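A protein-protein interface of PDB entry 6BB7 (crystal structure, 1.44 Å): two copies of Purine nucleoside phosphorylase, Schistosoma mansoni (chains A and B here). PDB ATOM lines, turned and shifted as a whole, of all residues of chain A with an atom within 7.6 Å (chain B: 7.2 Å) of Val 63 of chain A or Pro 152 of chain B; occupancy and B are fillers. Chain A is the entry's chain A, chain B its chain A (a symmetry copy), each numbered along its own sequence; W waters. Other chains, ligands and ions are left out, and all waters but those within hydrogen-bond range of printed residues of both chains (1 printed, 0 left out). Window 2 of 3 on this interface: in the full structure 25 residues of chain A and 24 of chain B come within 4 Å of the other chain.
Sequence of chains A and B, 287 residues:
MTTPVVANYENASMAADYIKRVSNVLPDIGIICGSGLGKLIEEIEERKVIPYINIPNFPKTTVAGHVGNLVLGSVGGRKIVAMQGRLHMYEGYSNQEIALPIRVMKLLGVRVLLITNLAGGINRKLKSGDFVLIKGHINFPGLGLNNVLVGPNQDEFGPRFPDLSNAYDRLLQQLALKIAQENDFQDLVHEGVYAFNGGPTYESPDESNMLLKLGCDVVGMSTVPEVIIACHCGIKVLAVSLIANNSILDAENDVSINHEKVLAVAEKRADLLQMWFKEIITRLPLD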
ATOM      1  N   LYS A  60       9.083  -0.395 -19.051  1.00  0.00           N
ATOM      2  CA  LYS A  60       9.044  -1.603 -18.234  1.00  0.00           C
ATOM      3  C   LYS A  60       7.631  -2.179 -18.222  1.00  0.00           C
ATOM      4  O   LYS A  60       6.659  -1.469 -17.948  1.00  0.00           O
ATOM      5  CB  LYS A  60       9.494  -1.283 -16.810  1.00  0.00           C
ATOM      6  CG  LYS A  60       9.547  -2.482 -15.858  1.00  0.00           C
ATOM      7  CD  LYS A  60      10.166  -2.050 -14.525  1.00  0.00           C
ATOM      8  CE  LYS A  60      10.233  -3.183 -13.511  1.00  0.00           C
ATOM      9  NZ  LYS A  60      11.081  -4.316 -13.986  1.00  0.00           N
ATOM     10  N   THR A  61       7.530  -3.496 -18.486  1.00  0.00           N
ATOM     11  CA  THR A  61       6.235  -4.161 -18.629  1.00  0.00           C
ATOM     12  C   THR A  61       6.084  -5.375 -17.711  1.00  0.00           C
ATOM     13  O   THR A  61       5.139  -6.154 -17.894  1.00  0.00           O
ATOM     14  CB  THR A  61       5.958  -4.551 -20.092  1.00  0.00           C
ATOM     15  OG1 THR A  61       6.825  -5.624 -20.494  1.00  0.00           O
ATOM     16  CG2 THR A  61       6.167  -3.362 -21.027  1.00  0.00           C
ATOM     17  N   THR A  62       6.953  -5.539 -16.702  1.00  0.00           N
ATOM     18  CA  THR A  62       6.929  -6.745 -15.886  1.00  0.00           C
ATOM     19  C   THR A  62       5.788  -6.776 -14.871  1.00  0.00           C
ATOM     20  O   THR A  62       5.453  -7.857 -14.391  1.00  0.00           O
ATOM     21  CB  THR A  62       8.277  -6.929 -15.181  1.00  0.00           C
ATOM     22  OG1 THR A  62       8.583  -5.751 -14.424  1.00  0.00           O
ATOM     23  CG2 THR A  62       9.389  -7.186 -16.210  1.00  0.00           C
ATOM     24  N   VAL A  63       5.164  -5.641 -14.529  1.00  0.00           N
ATOM     25  CA  VAL A  63       4.017  -5.728 -13.619  1.00  0.00           C
ATOM     26  C   VAL A  63       2.860  -6.429 -14.314  1.00  0.00           C
ATOM     27  O   VAL A  63       2.215  -7.317 -13.737  1.00  0.00           O
ATOM     28  CB  VAL A  63       3.632  -4.343 -13.049  1.00  0.00           C
ATOM     29  CG1 VAL A  63       2.384  -4.442 -12.172  1.00  0.00           C
ATOM     30  CG2 VAL A  63       4.792  -3.746 -12.224  1.00  0.00           C
ATOM     31  N   ALA A  64       2.600  -6.071 -15.578  1.00  0.00           N
ATOM     32  CA  ALA A  64       1.546  -6.753 -16.326  1.00  0.00           C
ATOM     33  C   ALA A  64       1.987  -8.146 -16.750  1.00  0.00           C
ATOM     34  O   ALA A  64       1.166  -9.073 -16.814  1.00  0.00           O
ATOM     35  CB  ALA A  64       1.180  -5.931 -17.561  1.00  0.00           C
ATOM     36  N   GLY A  65       3.281  -8.313 -17.022  1.00  0.00           N
ATOM     37  CA  GLY A  65       3.794  -9.573 -17.507  1.00  0.00           C
ATOM     38  C   GLY A  65       3.361  -9.831 -18.941  1.00  0.00           C
ATOM     39  O   GLY A  65       3.036  -8.921 -19.715  1.00  0.00           O
ATOM     40  N   HIS A  66       3.341 -11.119 -19.280  1.00  0.00           N
ATOM     41  CA  HIS A  66       3.004 -11.587 -20.622  1.00  0.00           C
ATOM     42  C   HIS A  66       4.004 -11.106 -21.676  1.00  0.00           C
ATOM     43  O   HIS A  66       4.980 -10.417 -21.350  1.00  0.00           O
ATOM     44  CB  HIS A  66       1.555 -11.216 -20.957  1.00  0.00           C
ATOM     45  CG  HIS A  66       0.556 -11.845 -20.037  1.00  0.00           C
ATOM     46  ND1 HIS A  66       0.093 -11.220 -18.898  1.00  0.00           N
ATOM     47  CD2 HIS A  66      -0.046 -13.057 -20.074  1.00  0.00           C
ATOM     48  CE1 HIS A  66      -0.759 -12.018 -18.277  1.00  0.00           C
ATOM     49  NE2 HIS A  66      -0.861 -13.139 -18.969  1.00  0.00           N
ATOM     50  N   TYR A  90      -5.081   1.727 -20.196  1.00  0.00           N
ATOM     51  CA  TYR A  90      -5.766   1.259 -18.983  1.00  0.00           C
ATOM     52  C   TYR A  90      -4.843   0.475 -18.042  1.00  0.00           C
ATOM     53  O   TYR A  90      -5.235   0.203 -16.899  1.00  0.00           O
ATOM     54  CB  TYR A  90      -7.034   0.436 -19.311  1.00  0.00           C
ATOM     55  CG  TYR A  90      -6.799  -0.789 -20.191  1.00  0.00           C
ATOM     56  CD1 TYR A  90      -6.179  -1.930 -19.682  1.00  0.00           C
ATOM     57  CD2 TYR A  90      -7.200  -0.813 -21.517  1.00  0.00           C
ATOM     58  CE1 TYR A  90      -5.938  -3.035 -20.485  1.00  0.00           C
ATOM     59  CE2 TYR A  90      -6.944  -1.915 -22.337  1.00  0.00           C
ATOM     60  CZ  TYR A  90      -6.325  -3.029 -21.814  1.00  0.00           C
ATOM     61  OH  TYR A  90      -6.118  -4.124 -22.638  1.00  0.00           O
ATOM     62  N   GLU A  91      -3.638   0.059 -18.485  1.00  0.00           N
ATOM     63  CA  GLU A  91      -2.702  -0.643 -17.605  1.00  0.00           C
ATOM     64  C   GLU A  91      -1.915   0.314 -16.721  1.00  0.00           C
ATOM     65  O   GLU A  91      -1.204  -0.169 -15.820  1.00  0.00           O
ATOM     66  CB  GLU A  91      -1.706  -1.443 -18.432  1.00  0.00           C
ATOM     67  CG  GLU A  91      -2.258  -2.656 -19.034  1.00  0.00           C
ATOM     68  CD  GLU A  91      -2.462  -3.844 -18.016  1.00  0.00           C
ATOM     69  OE1 GLU A  91      -1.865  -3.907 -16.900  1.00  0.00           O
ATOM     70  OE2 GLU A  91      -3.197  -4.786 -18.364  1.00  0.00           O
ATOM     71  N   GLY A  92      -2.033   1.616 -16.963  1.00  0.00           N
ATOM     72  CA  GLY A  92      -1.304   2.613 -16.212  1.00  0.00           C
ATOM     73  C   GLY A  92      -0.044   3.145 -16.865  1.00  0.00           C
ATOM     74  O   GLY A  92       0.642   3.961 -16.233  1.00  0.00           O
ATOM     75  N   TYR A  93       0.274   2.735 -18.095  1.00  0.00           N
ATOM     76  CA  TYR A  93       1.416   3.327 -18.805  1.00  0.00           C
ATOM     77  C   TYR A  93       1.181   4.814 -19.047  1.00  0.00           C
ATOM     78  O   TYR A  93       0.071   5.245 -19.373  1.00  0.00           O
ATOM     79  CB  TYR A  93       1.645   2.610 -20.141  1.00  0.00           C
ATOM     80  CG  TYR A  93       2.004   1.135 -19.981  1.00  0.00           C
ATOM     81  CD1 TYR A  93       3.176   0.732 -19.352  1.00  0.00           C
ATOM     82  CD2 TYR A  93       1.149   0.138 -20.431  1.00  0.00           C
ATOM     83  CE1 TYR A  93       3.497  -0.615 -19.193  1.00  0.00           C
ATOM     84  CE2 TYR A  93       1.455  -1.195 -20.280  1.00  0.00           C
ATOM     85  CZ  TYR A  93       2.633  -1.581 -19.649  1.00  0.00           C
ATOM     86  OH  TYR A  93       2.962  -2.893 -19.455  1.00  0.00           O
ATOM     87  N   VAL B   6      -0.476   0.054  -2.676  1.00  0.00           N
ATOM     88  CA  VAL B   6      -1.357  -0.532  -3.686  1.00  0.00           C
ATOM     89  C   VAL B   6      -2.487  -1.314  -3.016  1.00  0.00           C
ATOM     90  O   VAL B   6      -2.296  -1.946  -1.972  1.00  0.00           O
ATOM     91  CB  VAL B   6      -0.537  -1.406  -4.657  1.00  0.00           C
ATOM     92  CG1 VAL B   6      -1.414  -2.142  -5.694  1.00  0.00           C
ATOM     93  CG2 VAL B   6       0.528  -0.556  -5.366  1.00  0.00           C
ATOM     94  N   GLN B  96      -5.952   3.631  -5.936  1.00  0.00           N
ATOM     95  CA  GLN B  96      -5.578   2.635  -4.940  1.00  0.00           C
ATOM     96  C   GLN B  96      -6.147   2.973  -3.562  1.00  0.00           C
ATOM     97  O   GLN B  96      -6.516   2.060  -2.808  1.00  0.00           O
ATOM     98  CB  GLN B  96      -4.047   2.525  -4.860  1.00  0.00           C
ATOM     99  CG  GLN B  96      -3.272   2.217  -6.152  1.00  0.00           C
ATOM    100  CD  GLN B  96      -3.616   0.873  -6.748  1.00  0.00           C
ATOM    101  OE1 GLN B  96      -4.227   0.007  -6.120  1.00  0.00           O
ATOM    102  NE2 GLN B  96      -3.184   0.684  -8.007  1.00  0.00           N
ATOM    103  N   ARG B 103     -12.064  -3.497  -0.853  1.00  0.00           N
ATOM    104  CA  ARG B 103     -11.432  -4.827  -0.892  1.00  0.00           C
ATOM    105  C   ARG B 103     -11.235  -5.435   0.502  1.00  0.00           C
ATOM    106  O   ARG B 103     -11.344  -6.661   0.663  1.00  0.00           O
ATOM    107  CB  ARG B 103     -10.145  -4.753  -1.729  1.00  0.00           C
ATOM    108  CG  ARG B 103     -10.455  -4.583  -3.213  1.00  0.00           C
ATOM    109  CD  ARG B 103      -9.248  -4.369  -4.123  1.00  0.00           C
ATOM    110  NE  ARG B 103      -9.672  -4.351  -5.533  1.00  0.00           N
ATOM    111  CZ  ARG B 103      -8.922  -3.963  -6.552  1.00  0.00           C
ATOM    112  NH1 ARG B 103      -7.679  -3.546  -6.375  1.00  0.00           N
ATOM    113  NH2 ARG B 103      -9.428  -3.942  -7.788  1.00  0.00           N
ATOM    114  N   LEU B 149     -10.307   1.573 -12.028  1.00  0.00           N
ATOM    115  CA  LEU B 149      -9.522   0.358 -12.285  1.00  0.00           C
ATOM    116  C   LEU B 149      -8.300   0.582 -13.188  1.00  0.00           C
ATOM    117  O   LEU B 149      -7.585  -0.397 -13.489  1.00  0.00           O
ATOM    118  CB  LEU B 149     -10.416  -0.785 -12.854  1.00  0.00           C
ATOM    119  CG  LEU B 149     -11.370  -1.475 -11.854  1.00  0.00           C
ATOM    120  CD1 LEU B 149     -12.358  -2.345 -12.582  1.00  0.00           C
ATOM    121  CD2 LEU B 149     -10.593  -2.307 -10.803  1.00  0.00           C
ATOM    122  N   VAL B 150      -8.018   1.824 -13.637  1.00  0.00           N
ATOM    123  CA  VAL B 150      -6.779   2.059 -14.398  1.00  0.00           C
ATOM    124  C   VAL B 150      -5.576   1.735 -13.518  1.00  0.00           C
ATOM    125  O   VAL B 150      -5.454   2.250 -12.389  1.00  0.00           O
ATOM    126  CB  VAL B 150      -6.717   3.507 -14.916  1.00  0.00           C
ATOM    127  CG1 VAL B 150      -5.299   3.827 -15.443  1.00  0.00           C
ATOM    128  CG2 VAL B 150      -7.748   3.774 -16.010  1.00  0.00           C
ATOM    129  N   GLY B 151      -4.665   0.904 -14.044  1.00  0.00           N
ATOM    130  CA  GLY B 151      -3.522   0.372 -13.317  1.00  0.00           C
ATOM    131  C   GLY B 151      -3.422  -1.128 -13.553  1.00  0.00           C
ATOM    132  O   GLY B 151      -4.219  -1.710 -14.298  1.00  0.00           O
ATOM    133  N   PRO B 152      -2.433  -1.781 -12.945  1.00  0.00           N
ATOM    134  CA  PRO B 152      -2.390  -3.251 -13.005  1.00  0.00           C
ATOM    135  C   PRO B 152      -3.653  -3.861 -12.419  1.00  0.00           C
ATOM    136  O   PRO B 152      -4.234  -3.326 -11.467  1.00  0.00           O
ATOM    137  CB  PRO B 152      -1.163  -3.624 -12.171  1.00  0.00           C
ATOM    138  CG  PRO B 152      -0.744  -2.409 -11.458  1.00  0.00           C
ATOM    139  CD  PRO B 152      -1.409  -1.195 -12.075  1.00  0.00           C
ATOM    140  N   ASN B 153      -4.070  -5.003 -12.977  1.00  0.00           N
ATOM    141  CA  ASN B 153      -5.198  -5.730 -12.383  1.00  0.00           C
ATOM    142  C   ASN B 153      -4.740  -6.548 -11.165  1.00  0.00           C
ATOM    143  O   ASN B 153      -3.690  -7.209 -11.196  1.00  0.00           O
ATOM    144  CB  ASN B 153      -5.886  -6.664 -13.391  1.00  0.00           C
ATOM    145  CG  ASN B 153      -7.212  -7.224 -12.849  1.00  0.00           C
ATOM    146  OD1 ASN B 153      -8.118  -6.453 -12.471  1.00  0.00           O
ATOM    147  ND2 ASN B 153      -7.315  -8.544 -12.754  1.00  0.00           N
ATOM    148  N   GLN B 154      -5.548  -6.520 -10.096  1.00  0.00           N
ATOM    149  CA  GLN B 154      -5.332  -7.366  -8.918  1.00  0.00           C
ATOM    150  C   GLN B 154      -6.190  -8.626  -9.107  1.00  0.00           C
ATOM    151  O   GLN B 154      -7.381  -8.640  -8.783  1.00  0.00           O
ATOM    152  CB  GLN B 154      -5.629  -6.596  -7.631  1.00  0.00           C
ATOM    153  CG  GLN B 154      -4.819  -5.288  -7.509  1.00  0.00           C
ATOM    154  CD  GLN B 154      -3.311  -5.489  -7.520  1.00  0.00           C
ATOM    155  OE1 GLN B 154      -2.782  -6.534  -7.104  1.00  0.00           O
ATOM    156  NE2 GLN B 154      -2.597  -4.483  -8.023  1.00  0.00           N
ATOM    157  N   ASP B 155      -5.558  -9.672  -9.682  1.00  0.00           N
ATOM    158  CA  ASP B 155      -6.259 -10.878 -10.157  1.00  0.00           C
ATOM    159  C   ASP B 155      -7.007 -11.620  -9.049  1.00  0.00           C
ATOM    160  O   ASP B 155      -8.060 -12.227  -9.305  1.00  0.00           O
ATOM    161  CB  ASP B 155      -5.255 -11.832 -10.821  1.00  0.00           C
ATOM    162  CG  ASP B 155      -4.611 -11.235 -12.074  1.00  0.00           C
ATOM    163  OD1 ASP B 155      -5.323 -10.603 -12.904  1.00  0.00           O
ATOM    164  OD2 ASP B 155      -3.378 -11.433 -12.277  1.00  0.00           O
ATOM    165  N   ARG B 160      -9.606  -8.694 -15.472  1.00  0.00           N
ATOM    166  CA  ARG B 160      -9.016  -7.517 -16.119  1.00  0.00           C
ATOM    167  C   ARG B 160     -10.082  -6.608 -16.737  1.00  0.00           C
ATOM    168  O   ARG B 160      -9.979  -5.362 -16.635  1.00  0.00           O
ATOM    169  CB  ARG B 160      -7.959  -7.947 -17.154  1.00  0.00           C
ATOM    170  CG  ARG B 160      -7.399  -6.846 -18.104  1.00  0.00           C
ATOM    171  CD  ARG B 160      -6.365  -5.925 -17.445  1.00  0.00           C
ATOM    172  NE  ARG B 160      -6.939  -4.945 -16.524  1.00  0.00           N
ATOM    173  CZ  ARG B 160      -6.260  -3.939 -15.971  1.00  0.00           C
ATOM    174  NH1 ARG B 160      -6.853  -3.110 -15.112  1.00  0.00           N
ATOM    175  NH2 ARG B 160      -4.962  -3.772 -16.231  1.00  0.00           N
HETATM  176  O   HOH W   1      -0.873  -7.272 -12.762  1.00  0.00           O
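O of Tyr 90 of chain A is in hydrogen-bond range of N of Gly 151 of chain B (3.0 Å).
NH2 of Arg 160 of chain B is in salt-bridge range of OE2 of Glu 91 of chain A.
The backbone carbonyl oxygen (O) of Leu 149 of chain B lies within hydrogen-bond range of the guanidinium group (NH1) of Arg 160 of chain B (3.2 Å).
The guanidinium group (NH2) of Arg 160 of chain B is in hydrogen-bond range of the backbone carbonyl oxygen (O) of Gly 151 of chain B (2.9 Å).
CB of Pro 152 of chain B touches CG1 of Val 63 of chain A, 3.6 Å away.
CA of Val 150 of chain B touches O of Tyr 90 of chain A, 3.5 Å away.
C of Gly 151 of chain B touches O of Glu 91 of chain A (3.3 Å).
O of Glu 91 of chain A touches N of Pro 152 of chain B (3.5 Å).
Gly 92 of chain A touches Gly 151 of chain B.
Val 63 of chain A touches just one residue of chain B: Pro 152 (3.6 Å).
Of the printed residues of chain B, Tyr 90 of chain A touches Val 150 (3.5 Å) and Gly 151 (3.0 Å).
Of the printed residues of chain B, Glu 91 of chain A touches Gly 151, Pro 152 and Arg 160.
Of the printed residues of chain B, Gly 92 of chain A touches Gly 151 (3.99 Å).
Of the printed residues of chain A, Gly 151 of chain B touches Tyr 90 (3.0 Å), Glu 91 (3.3 Å) and Gly 92 (3.99 Å).
Of chain A, only Val 63 and Glu 91 come within 4 Å of Pro 152 of chain B.
Asn 153 of chain B touches none of the printed residues of chain A.
Printed residues of chain A within 4 Å of Arg 160 of chain B: Glu 91.
The nearest residue of chain B that does not touch Val 63 of chain A is Asn 153 of chain B (6.4 Å).
Printed residues of chain A that touch a printed residue of chain B: Val 63, Tyr 90, Glu 91 and Gly 92.
Hydrophobic or aromatic side chains of chain A that line the printed part of chain B: Val 63.
Of the 11 printed residues of chain B, 4 touch a printed residue of chain A.
Along chain B the printed residues that touch a printed residue of chain A span positions 150 to 160.
Among the printed residues, 7 pairs touch across the chains.
Among the printed residues, Asp or Glu carboxylates within 4 Å of a Lys or Arg side-chain nitrogen of the other chain: Glu 91 of chain A with Arg 160 of chain B.
No position is printed for both chains.
Of the 7 pairs that touch across the chains among the printed residues, none has its exchanged pair printed and touching as well.
Water W1 lies within hydrogen-bond range of the backbone carbonyl oxygen (O) of Asn 153 of chain B (3.2 Å) and the backbone carbonyl oxygen (O) of Val 63 of chain A (3.2 Å).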
